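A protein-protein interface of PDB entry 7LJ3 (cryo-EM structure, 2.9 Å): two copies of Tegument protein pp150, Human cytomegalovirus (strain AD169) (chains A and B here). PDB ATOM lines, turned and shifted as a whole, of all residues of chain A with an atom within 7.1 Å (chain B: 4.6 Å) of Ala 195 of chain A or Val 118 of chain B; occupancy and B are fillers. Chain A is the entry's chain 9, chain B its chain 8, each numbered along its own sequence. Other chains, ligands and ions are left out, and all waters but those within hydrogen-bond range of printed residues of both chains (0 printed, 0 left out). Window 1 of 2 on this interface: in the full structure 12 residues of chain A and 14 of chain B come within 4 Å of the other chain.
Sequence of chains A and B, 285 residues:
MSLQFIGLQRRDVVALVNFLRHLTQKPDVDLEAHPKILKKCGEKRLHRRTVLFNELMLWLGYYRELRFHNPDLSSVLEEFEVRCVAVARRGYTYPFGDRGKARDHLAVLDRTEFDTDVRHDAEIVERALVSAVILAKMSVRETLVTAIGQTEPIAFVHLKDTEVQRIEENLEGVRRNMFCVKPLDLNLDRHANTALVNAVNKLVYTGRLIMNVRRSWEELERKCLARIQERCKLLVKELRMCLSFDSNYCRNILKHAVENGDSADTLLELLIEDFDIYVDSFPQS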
ATOM      1  N   ALA A  86     -13.444  16.045 -24.797  1.00  0.00           N
ATOM      2  CA  ALA A  86     -12.248  15.464 -24.191  1.00  0.00           C
ATOM      3  C   ALA A  86     -12.571  14.199 -23.402  1.00  0.00           C
ATOM      4  O   ALA A  86     -11.842  13.197 -23.479  1.00  0.00           O
ATOM      5  CB  ALA A  86     -11.579  16.496 -23.286  1.00  0.00           C
ATOM      6  N   VAL A  87     -13.652  14.232 -22.624  1.00  0.00           N
ATOM      7  CA  VAL A  87     -14.095  13.036 -21.913  1.00  0.00           C
ATOM      8  C   VAL A  87     -14.382  11.921 -22.905  1.00  0.00           C
ATOM      9  O   VAL A  87     -13.999  10.761 -22.696  1.00  0.00           O
ATOM     10  CB  VAL A  87     -15.329  13.360 -21.049  1.00  0.00           C
ATOM     11  CG1 VAL A  87     -15.760  12.154 -20.254  1.00  0.00           C
ATOM     12  CG2 VAL A  87     -15.039  14.527 -20.130  1.00  0.00           C
ATOM     13  N   ARG A  90     -11.153  10.350 -24.185  1.00  0.00           N
ATOM     14  CA  ARG A  90     -10.524   9.417 -23.256  1.00  0.00           C
ATOM     15  C   ARG A  90     -11.302   8.110 -23.168  1.00  0.00           C
ATOM     16  O   ARG A  90     -10.709   7.039 -23.000  1.00  0.00           O
ATOM     17  CB  ARG A  90     -10.372  10.044 -21.876  1.00  0.00           C
ATOM     18  CG  ARG A  90      -9.201  10.984 -21.784  1.00  0.00           C
ATOM     19  CD  ARG A  90      -8.014  10.419 -22.525  1.00  0.00           C
ATOM     20  NE  ARG A  90      -7.010  11.442 -22.776  1.00  0.00           N
ATOM     21  CZ  ARG A  90      -5.898  11.248 -23.474  1.00  0.00           C
ATOM     22  NH1 ARG A  90      -5.638  10.065 -24.002  1.00  0.00           N
ATOM     23  NH2 ARG A  90      -5.046  12.241 -23.647  1.00  0.00           N
ATOM     24  N   ASP A 189      -7.272  16.778 -10.842  1.00  0.00           N
ATOM     25  CA  ASP A 189      -6.475  15.659 -11.329  1.00  0.00           C
ATOM     26  C   ASP A 189      -5.759  14.967 -10.179  1.00  0.00           C
ATOM     27  O   ASP A 189      -5.189  15.617  -9.301  1.00  0.00           O
ATOM     28  CB  ASP A 189      -5.462  16.129 -12.370  1.00  0.00           C
ATOM     29  CG  ASP A 189      -6.098  16.426 -13.714  1.00  0.00           C
ATOM     30  OD1 ASP A 189      -7.313  16.698 -13.753  1.00  0.00           O
ATOM     31  OD2 ASP A 189      -5.384  16.378 -14.733  1.00  0.00           O
ATOM     32  N   ARG A 190      -5.803  13.641 -10.193  1.00  0.00           N
ATOM     33  CA  ARG A 190      -5.248  12.793  -9.154  1.00  0.00           C
ATOM     34  C   ARG A 190      -4.445  11.686  -9.821  1.00  0.00           C
ATOM     35  O   ARG A 190      -4.853  11.164 -10.860  1.00  0.00           O
ATOM     36  CB  ARG A 190      -6.377  12.231  -8.293  1.00  0.00           C
ATOM     37  CG  ARG A 190      -5.963  11.403  -7.127  1.00  0.00           C
ATOM     38  CD  ARG A 190      -7.002  11.478  -6.024  1.00  0.00           C
ATOM     39  NE  ARG A 190      -6.769  10.427  -5.045  1.00  0.00           N
ATOM     40  CZ  ARG A 190      -5.768  10.441  -4.177  1.00  0.00           C
ATOM     41  NH1 ARG A 190      -5.602   9.440  -3.329  1.00  0.00           N
ATOM     42  NH2 ARG A 190      -4.927  11.463  -4.172  1.00  0.00           N
ATOM     43  N   HIS A 191      -3.288  11.343  -9.250  1.00  0.00           N
ATOM     44  CA  HIS A 191      -2.470  10.288  -9.847  1.00  0.00           C
ATOM     45  C   HIS A 191      -3.195   8.950  -9.820  1.00  0.00           C
ATOM     46  O   HIS A 191      -3.171   8.200 -10.801  1.00  0.00           O
ATOM     47  CB  HIS A 191      -1.120  10.186  -9.129  1.00  0.00           C
ATOM     48  CG  HIS A 191      -0.153   9.245  -9.781  1.00  0.00           C
ATOM     49  ND1 HIS A 191       0.114   7.988  -9.284  1.00  0.00           N
ATOM     50  CD2 HIS A 191       0.629   9.388 -10.875  1.00  0.00           C
ATOM     51  CE1 HIS A 191       1.001   7.390 -10.057  1.00  0.00           C
ATOM     52  NE2 HIS A 191       1.332   8.220 -11.028  1.00  0.00           N
ATOM     53  N   ASN A 193      -6.368   8.328  -9.875  1.00  0.00           N
ATOM     54  CA  ASN A 193      -7.469   8.288 -10.822  1.00  0.00           C
ATOM     55  C   ASN A 193      -6.959   8.244 -12.259  1.00  0.00           C
ATOM     56  O   ASN A 193      -5.873   8.728 -12.583  1.00  0.00           O
ATOM     57  CB  ASN A 193      -8.388   9.495 -10.649  1.00  0.00           C
ATOM     58  CG  ASN A 193      -8.995   9.572  -9.275  1.00  0.00           C
ATOM     59  OD1 ASN A 193      -8.877   8.645  -8.484  1.00  0.00           O
ATOM     60  ND2 ASN A 193      -9.645  10.686  -8.977  1.00  0.00           N
ATOM     61  N   THR A 194      -7.780   7.658 -13.127  1.00  0.00           N
ATOM     62  CA  THR A 194      -7.471   7.561 -14.542  1.00  0.00           C
ATOM     63  C   THR A 194      -7.704   8.897 -15.235  1.00  0.00           C
ATOM     64  O   THR A 194      -8.351   9.798 -14.701  1.00  0.00           O
ATOM     65  CB  THR A 194      -8.326   6.483 -15.208  1.00  0.00           C
ATOM     66  OG1 THR A 194      -9.708   6.798 -15.037  1.00  0.00           O
ATOM     67  CG2 THR A 194      -8.058   5.137 -14.582  1.00  0.00           C
ATOM     68  N   ALA A 195      -7.176   9.015 -16.449  1.00  0.00           N
ATOM     69  CA  ALA A 195      -7.457  10.202 -17.245  1.00  0.00           C
ATOM     70  C   ALA A 195      -8.956  10.392 -17.430  1.00  0.00           C
ATOM     71  O   ALA A 195      -9.459  11.521 -17.375  1.00  0.00           O
ATOM     72  CB  ALA A 195      -6.747  10.111 -18.592  1.00  0.00           C
ATOM     73  N   LEU A 196      -9.689   9.297 -17.632  1.00  0.00           N
ATOM     74  CA  LEU A 196     -11.134   9.391 -17.784  1.00  0.00           C
ATOM     75  C   LEU A 196     -11.790   9.954 -16.532  1.00  0.00           C
ATOM     76  O   LEU A 196     -12.662  10.826 -16.621  1.00  0.00           O
ATOM     77  CB  LEU A 196     -11.709   8.017 -18.128  1.00  0.00           C
ATOM     78  CG  LEU A 196     -13.195   7.913 -18.494  1.00  0.00           C
ATOM     79  CD1 LEU A 196     -13.367   7.143 -19.774  1.00  0.00           C
ATOM     80  CD2 LEU A 196     -13.974   7.254 -17.394  1.00  0.00           C
ATOM     81  N   VAL A 197     -11.384   9.477 -15.352  1.00  0.00           N
ATOM     82  CA  VAL A 197     -11.989   9.964 -14.114  1.00  0.00           C
ATOM     83  C   VAL A 197     -11.697  11.446 -13.920  1.00  0.00           C
ATOM     84  O   VAL A 197     -12.563  12.214 -13.487  1.00  0.00           O
ATOM     85  CB  VAL A 197     -11.511   9.124 -12.916  1.00  0.00           C
ATOM     86  CG1 VAL A 197     -12.029   9.710 -11.629  1.00  0.00           C
ATOM     87  CG2 VAL A 197     -11.974   7.685 -13.054  1.00  0.00           C
ATOM     88  N   ASN A 198     -10.479  11.876 -14.253  1.00  0.00           N
ATOM     89  CA  ASN A 198     -10.117  13.283 -14.102  1.00  0.00           C
ATOM     90  C   ASN A 198     -10.912  14.174 -15.049  1.00  0.00           C
ATOM     91  O   ASN A 198     -11.397  15.243 -14.653  1.00  0.00           O
ATOM     92  CB  ASN A 198      -8.618  13.457 -14.331  1.00  0.00           C
ATOM     93  CG  ASN A 198      -7.789  12.767 -13.281  1.00  0.00           C
ATOM     94  OD1 ASN A 198      -8.264  12.493 -12.183  1.00  0.00           O
ATOM     95  ND2 ASN A 198      -6.536  12.488 -13.606  1.00  0.00           N
ATOM     96  N   ALA A 199     -11.050  13.755 -16.308  1.00  0.00           N
ATOM     97  CA  ALA A 199     -11.868  14.515 -17.245  1.00  0.00           C
ATOM     98  C   ALA A 199     -13.304  14.595 -16.764  1.00  0.00           C
ATOM     99  O   ALA A 199     -13.942  15.651 -16.854  1.00  0.00           O
ATOM    100  CB  ALA A 199     -11.800  13.890 -18.634  1.00  0.00           C
ATOM    101  N   VAL A 200     -13.834  13.485 -16.250  1.00  0.00           N
ATOM    102  CA  VAL A 200     -15.208  13.485 -15.764  1.00  0.00           C
ATOM    103  C   VAL A 200     -15.368  14.466 -14.612  1.00  0.00           C
ATOM    104  O   VAL A 200     -16.369  15.185 -14.526  1.00  0.00           O
ATOM    105  CB  VAL A 200     -15.628  12.061 -15.363  1.00  0.00           C
ATOM    106  CG1 VAL A 200     -16.904  12.089 -14.547  1.00  0.00           C
ATOM    107  CG2 VAL A 200     -15.802  11.209 -16.598  1.00  0.00           C
ATOM    108  N   ASN A 201     -14.385  14.518 -13.713  1.00  0.00           N
ATOM    109  CA  ASN A 201     -14.480  15.418 -12.567  1.00  0.00           C
ATOM    110  C   ASN A 201     -14.442  16.879 -12.998  1.00  0.00           C
ATOM    111  O   ASN A 201     -15.223  17.704 -12.504  1.00  0.00           O
ATOM    112  CB  ASN A 201     -13.359  15.127 -11.579  1.00  0.00           C
ATOM    113  CG  ASN A 201     -13.580  13.848 -10.813  1.00  0.00           C
ATOM    114  OD1 ASN A 201     -14.706  13.514 -10.451  1.00  0.00           O
ATOM    115  ND2 ASN A 201     -12.501  13.123 -10.556  1.00  0.00           N
ATOM    116  N   THR B 116      -6.339   5.701 -23.602  1.00  0.00           N
ATOM    117  CA  THR B 116      -6.740   6.234 -22.306  1.00  0.00           C
ATOM    118  C   THR B 116      -5.595   6.974 -21.631  1.00  0.00           C
ATOM    119  O   THR B 116      -5.820   7.899 -20.844  1.00  0.00           O
ATOM    120  CB  THR B 116      -7.233   5.108 -21.404  1.00  0.00           C
ATOM    121  OG1 THR B 116      -8.120   4.256 -22.137  1.00  0.00           O
ATOM    122  CG2 THR B 116      -7.963   5.686 -20.197  1.00  0.00           C
ATOM    123  N   ASP B 117      -4.361   6.554 -21.891  1.00  0.00           N
ATOM    124  CA  ASP B 117      -3.208   7.135 -21.222  1.00  0.00           C
ATOM    125  C   ASP B 117      -2.773   8.422 -21.913  1.00  0.00           C
ATOM    126  O   ASP B 117      -2.630   8.461 -23.138  1.00  0.00           O
ATOM    127  CB  ASP B 117      -2.069   6.122 -21.203  1.00  0.00           C
ATOM    128  CG  ASP B 117      -1.053   6.404 -20.120  1.00  0.00           C
ATOM    129  OD1 ASP B 117      -1.228   7.386 -19.366  1.00  0.00           O
ATOM    130  OD2 ASP B 117      -0.080   5.632 -20.020  1.00  0.00           O
ATOM    131  N   VAL B 118      -2.573   9.482 -21.126  1.00  0.00           N
ATOM    132  CA  VAL B 118      -2.076  10.738 -21.682  1.00  0.00           C
ATOM    133  C   VAL B 118      -0.581  10.648 -21.961  1.00  0.00           C
ATOM    134  O   VAL B 118      -0.045  11.385 -22.796  1.00  0.00           O
ATOM    135  CB  VAL B 118      -2.407  11.916 -20.752  1.00  0.00           C
ATOM    136  CG1 VAL B 118      -3.900  12.016 -20.551  1.00  0.00           C
ATOM    137  CG2 VAL B 118      -1.694  11.757 -19.431  1.00  0.00           C
ATOM    138  N   ARG B 119       0.122   9.773 -21.243  1.00  0.00           N
ATOM    139  CA  ARG B 119       1.539   9.576 -21.511  1.00  0.00           C
ATOM    140  C   ARG B 119       1.778   8.976 -22.888  1.00  0.00           C
ATOM    141  O   ARG B 119       2.873   9.112 -23.441  1.00  0.00           O
ATOM    142  CB  ARG B 119       2.155   8.698 -20.429  1.00  0.00           C
ATOM    143  CG  ARG B 119       2.364   9.425 -19.125  1.00  0.00           C
ATOM    144  CD  ARG B 119       3.005   8.524 -18.100  1.00  0.00           C
ATOM    145  NE  ARG B 119       3.489   9.269 -16.944  1.00  0.00           N
ATOM    146  CZ  ARG B 119       2.840   9.360 -15.791  1.00  0.00           C
ATOM    147  NH1 ARG B 119       1.678   8.747 -15.640  1.00  0.00           N
ATOM    148  NH2 ARG B 119       3.357  10.057 -14.793  1.00  0.00           N
ATOM    149  N   HIS B 120       0.784   8.291 -23.451  1.00  0.00           N
ATOM    150  CA  HIS B 120       0.963   7.701 -24.771  1.00  0.00           C
ATOM    151  C   HIS B 120       0.851   8.723 -25.891  1.00  0.00           C
ATOM    152  O   HIS B 120       1.354   8.472 -26.990  1.00  0.00           O
ATOM    153  CB  HIS B 120      -0.048   6.583 -24.992  1.00  0.00           C
ATOM    154  CG  HIS B 120       0.267   5.325 -24.247  1.00  0.00           C
ATOM    155  ND1 HIS B 120       0.500   5.300 -22.890  1.00  0.00           N
ATOM    156  CD2 HIS B 120       0.376   4.044 -24.668  1.00  0.00           C
ATOM    157  CE1 HIS B 120       0.746   4.060 -22.509  1.00  0.00           C
ATOM    158  NE2 HIS B 120       0.672   3.277 -23.569  1.00  0.00           N
ATOM    159  N   ASP B 121       0.219   9.871 -25.639  1.00  0.00           N
ATOM    160  CA  ASP B 121      -0.041  10.821 -26.716  1.00  0.00           C
ATOM    161  C   ASP B 121       1.229  11.188 -27.464  1.00  0.00           C
ATOM    162  O   ASP B 121       1.192  11.398 -28.680  1.00  0.00           O
ATOM    163  CB  ASP B 121      -0.683  12.089 -26.163  1.00  0.00           C
ATOM    164  CG  ASP B 121      -1.845  11.802 -25.248  1.00  0.00           C
ATOM    165  OD1 ASP B 121      -2.132  10.615 -24.985  1.00  0.00           O
ATOM    166  OD2 ASP B 121      -2.482  12.771 -24.792  1.00  0.00           O
ATOM    167  N   ARG B 214       4.488  17.660 -24.321  1.00  0.00           N
ATOM    168  CA  ARG B 214       4.427  16.465 -23.482  1.00  0.00           C
ATOM    169  C   ARG B 214       5.805  16.064 -22.970  1.00  0.00           C
ATOM    170  O   ARG B 214       5.980  15.804 -21.770  1.00  0.00           O
ATOM    171  CB  ARG B 214       3.781  15.321 -24.263  1.00  0.00           C
ATOM    172  CG  ARG B 214       2.338  15.568 -24.675  1.00  0.00           C
ATOM    173  CD  ARG B 214       1.443  15.645 -23.468  1.00  0.00           C
ATOM    174  NE  ARG B 214       0.048  15.858 -23.833  1.00  0.00           N
ATOM    175  CZ  ARG B 214      -0.910  16.189 -22.975  1.00  0.00           C
ATOM    176  NH1 ARG B 214      -0.627  16.347 -21.692  1.00  0.00           N
ATOM    177  NH2 ARG B 214      -2.150  16.364 -23.404  1.00  0.00           N
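OD1 of Asp 117 of chain B lies close to N of Arg 119 of chain B (3.3 Å).
The side-chain carboxylate of Asp 117 of chain B sits at hydrogen-bond distance from a ring nitrogen (ND1) of His 120 of chain B (2.9 Å).
NH2 of Arg 214 of chain B is in salt-bridge range of OD2 of Asp 121 of chain B (3.9 Å).
Ala 195 of chain A touches just these residues of chain B: Thr 116 and Val 118.
Val 118 of chain B touches just these residues of chain A: Arg 90 (3.3 Å) and Ala 195 (3.9 Å).
Of the printed residues of chain A, Asp 117 of chain B touches Arg 90 (3.5 Å).
Of the printed residues of chain A, Asp 121 of chain B touches Arg 90.
The nearest printed residue of chain A that does not touch Asp 117 of chain B is Ala 195 of chain A (5.3 Å).
NH2 of Arg 90 of chain A is in salt-bridge range of OD2 of Asp 121 of chain B (2.9 Å).
Hydrophobic or aromatic side chains of chain A within 4 Å of the printed part of chain B: Ala 195.
Of the 7 printed residues of chain B, 4 touch a printed residue of chain A.
Hydrophobic or aromatic side chains of chain B within 4 Å of the printed part of chain A: Val 118.
Among the printed residues, 6 pairs touch across the chains.
Among the printed residues, Asp or Glu carboxylates within 4 Å of a Lys or Arg side-chain nitrogen of the other chain: Arg 90 of chain A with Asp 121 of chain B.
Thr 116 of chain B touches Arg 90 of chain A.
Arg 90 of chain A touches Asp 117 of chain B.
NH2 of Arg 90 of chain A touches CG1 of Val 118 of chain B, 3.3 Å away.
Ala 195 of chain A touches Thr 116 of chain B (CB to O, 3.3 Å).
Val 118 of chain B touches Ala 195 of chain A (CG1 to CB, 3.9 Å).
No position is printed for both chains.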
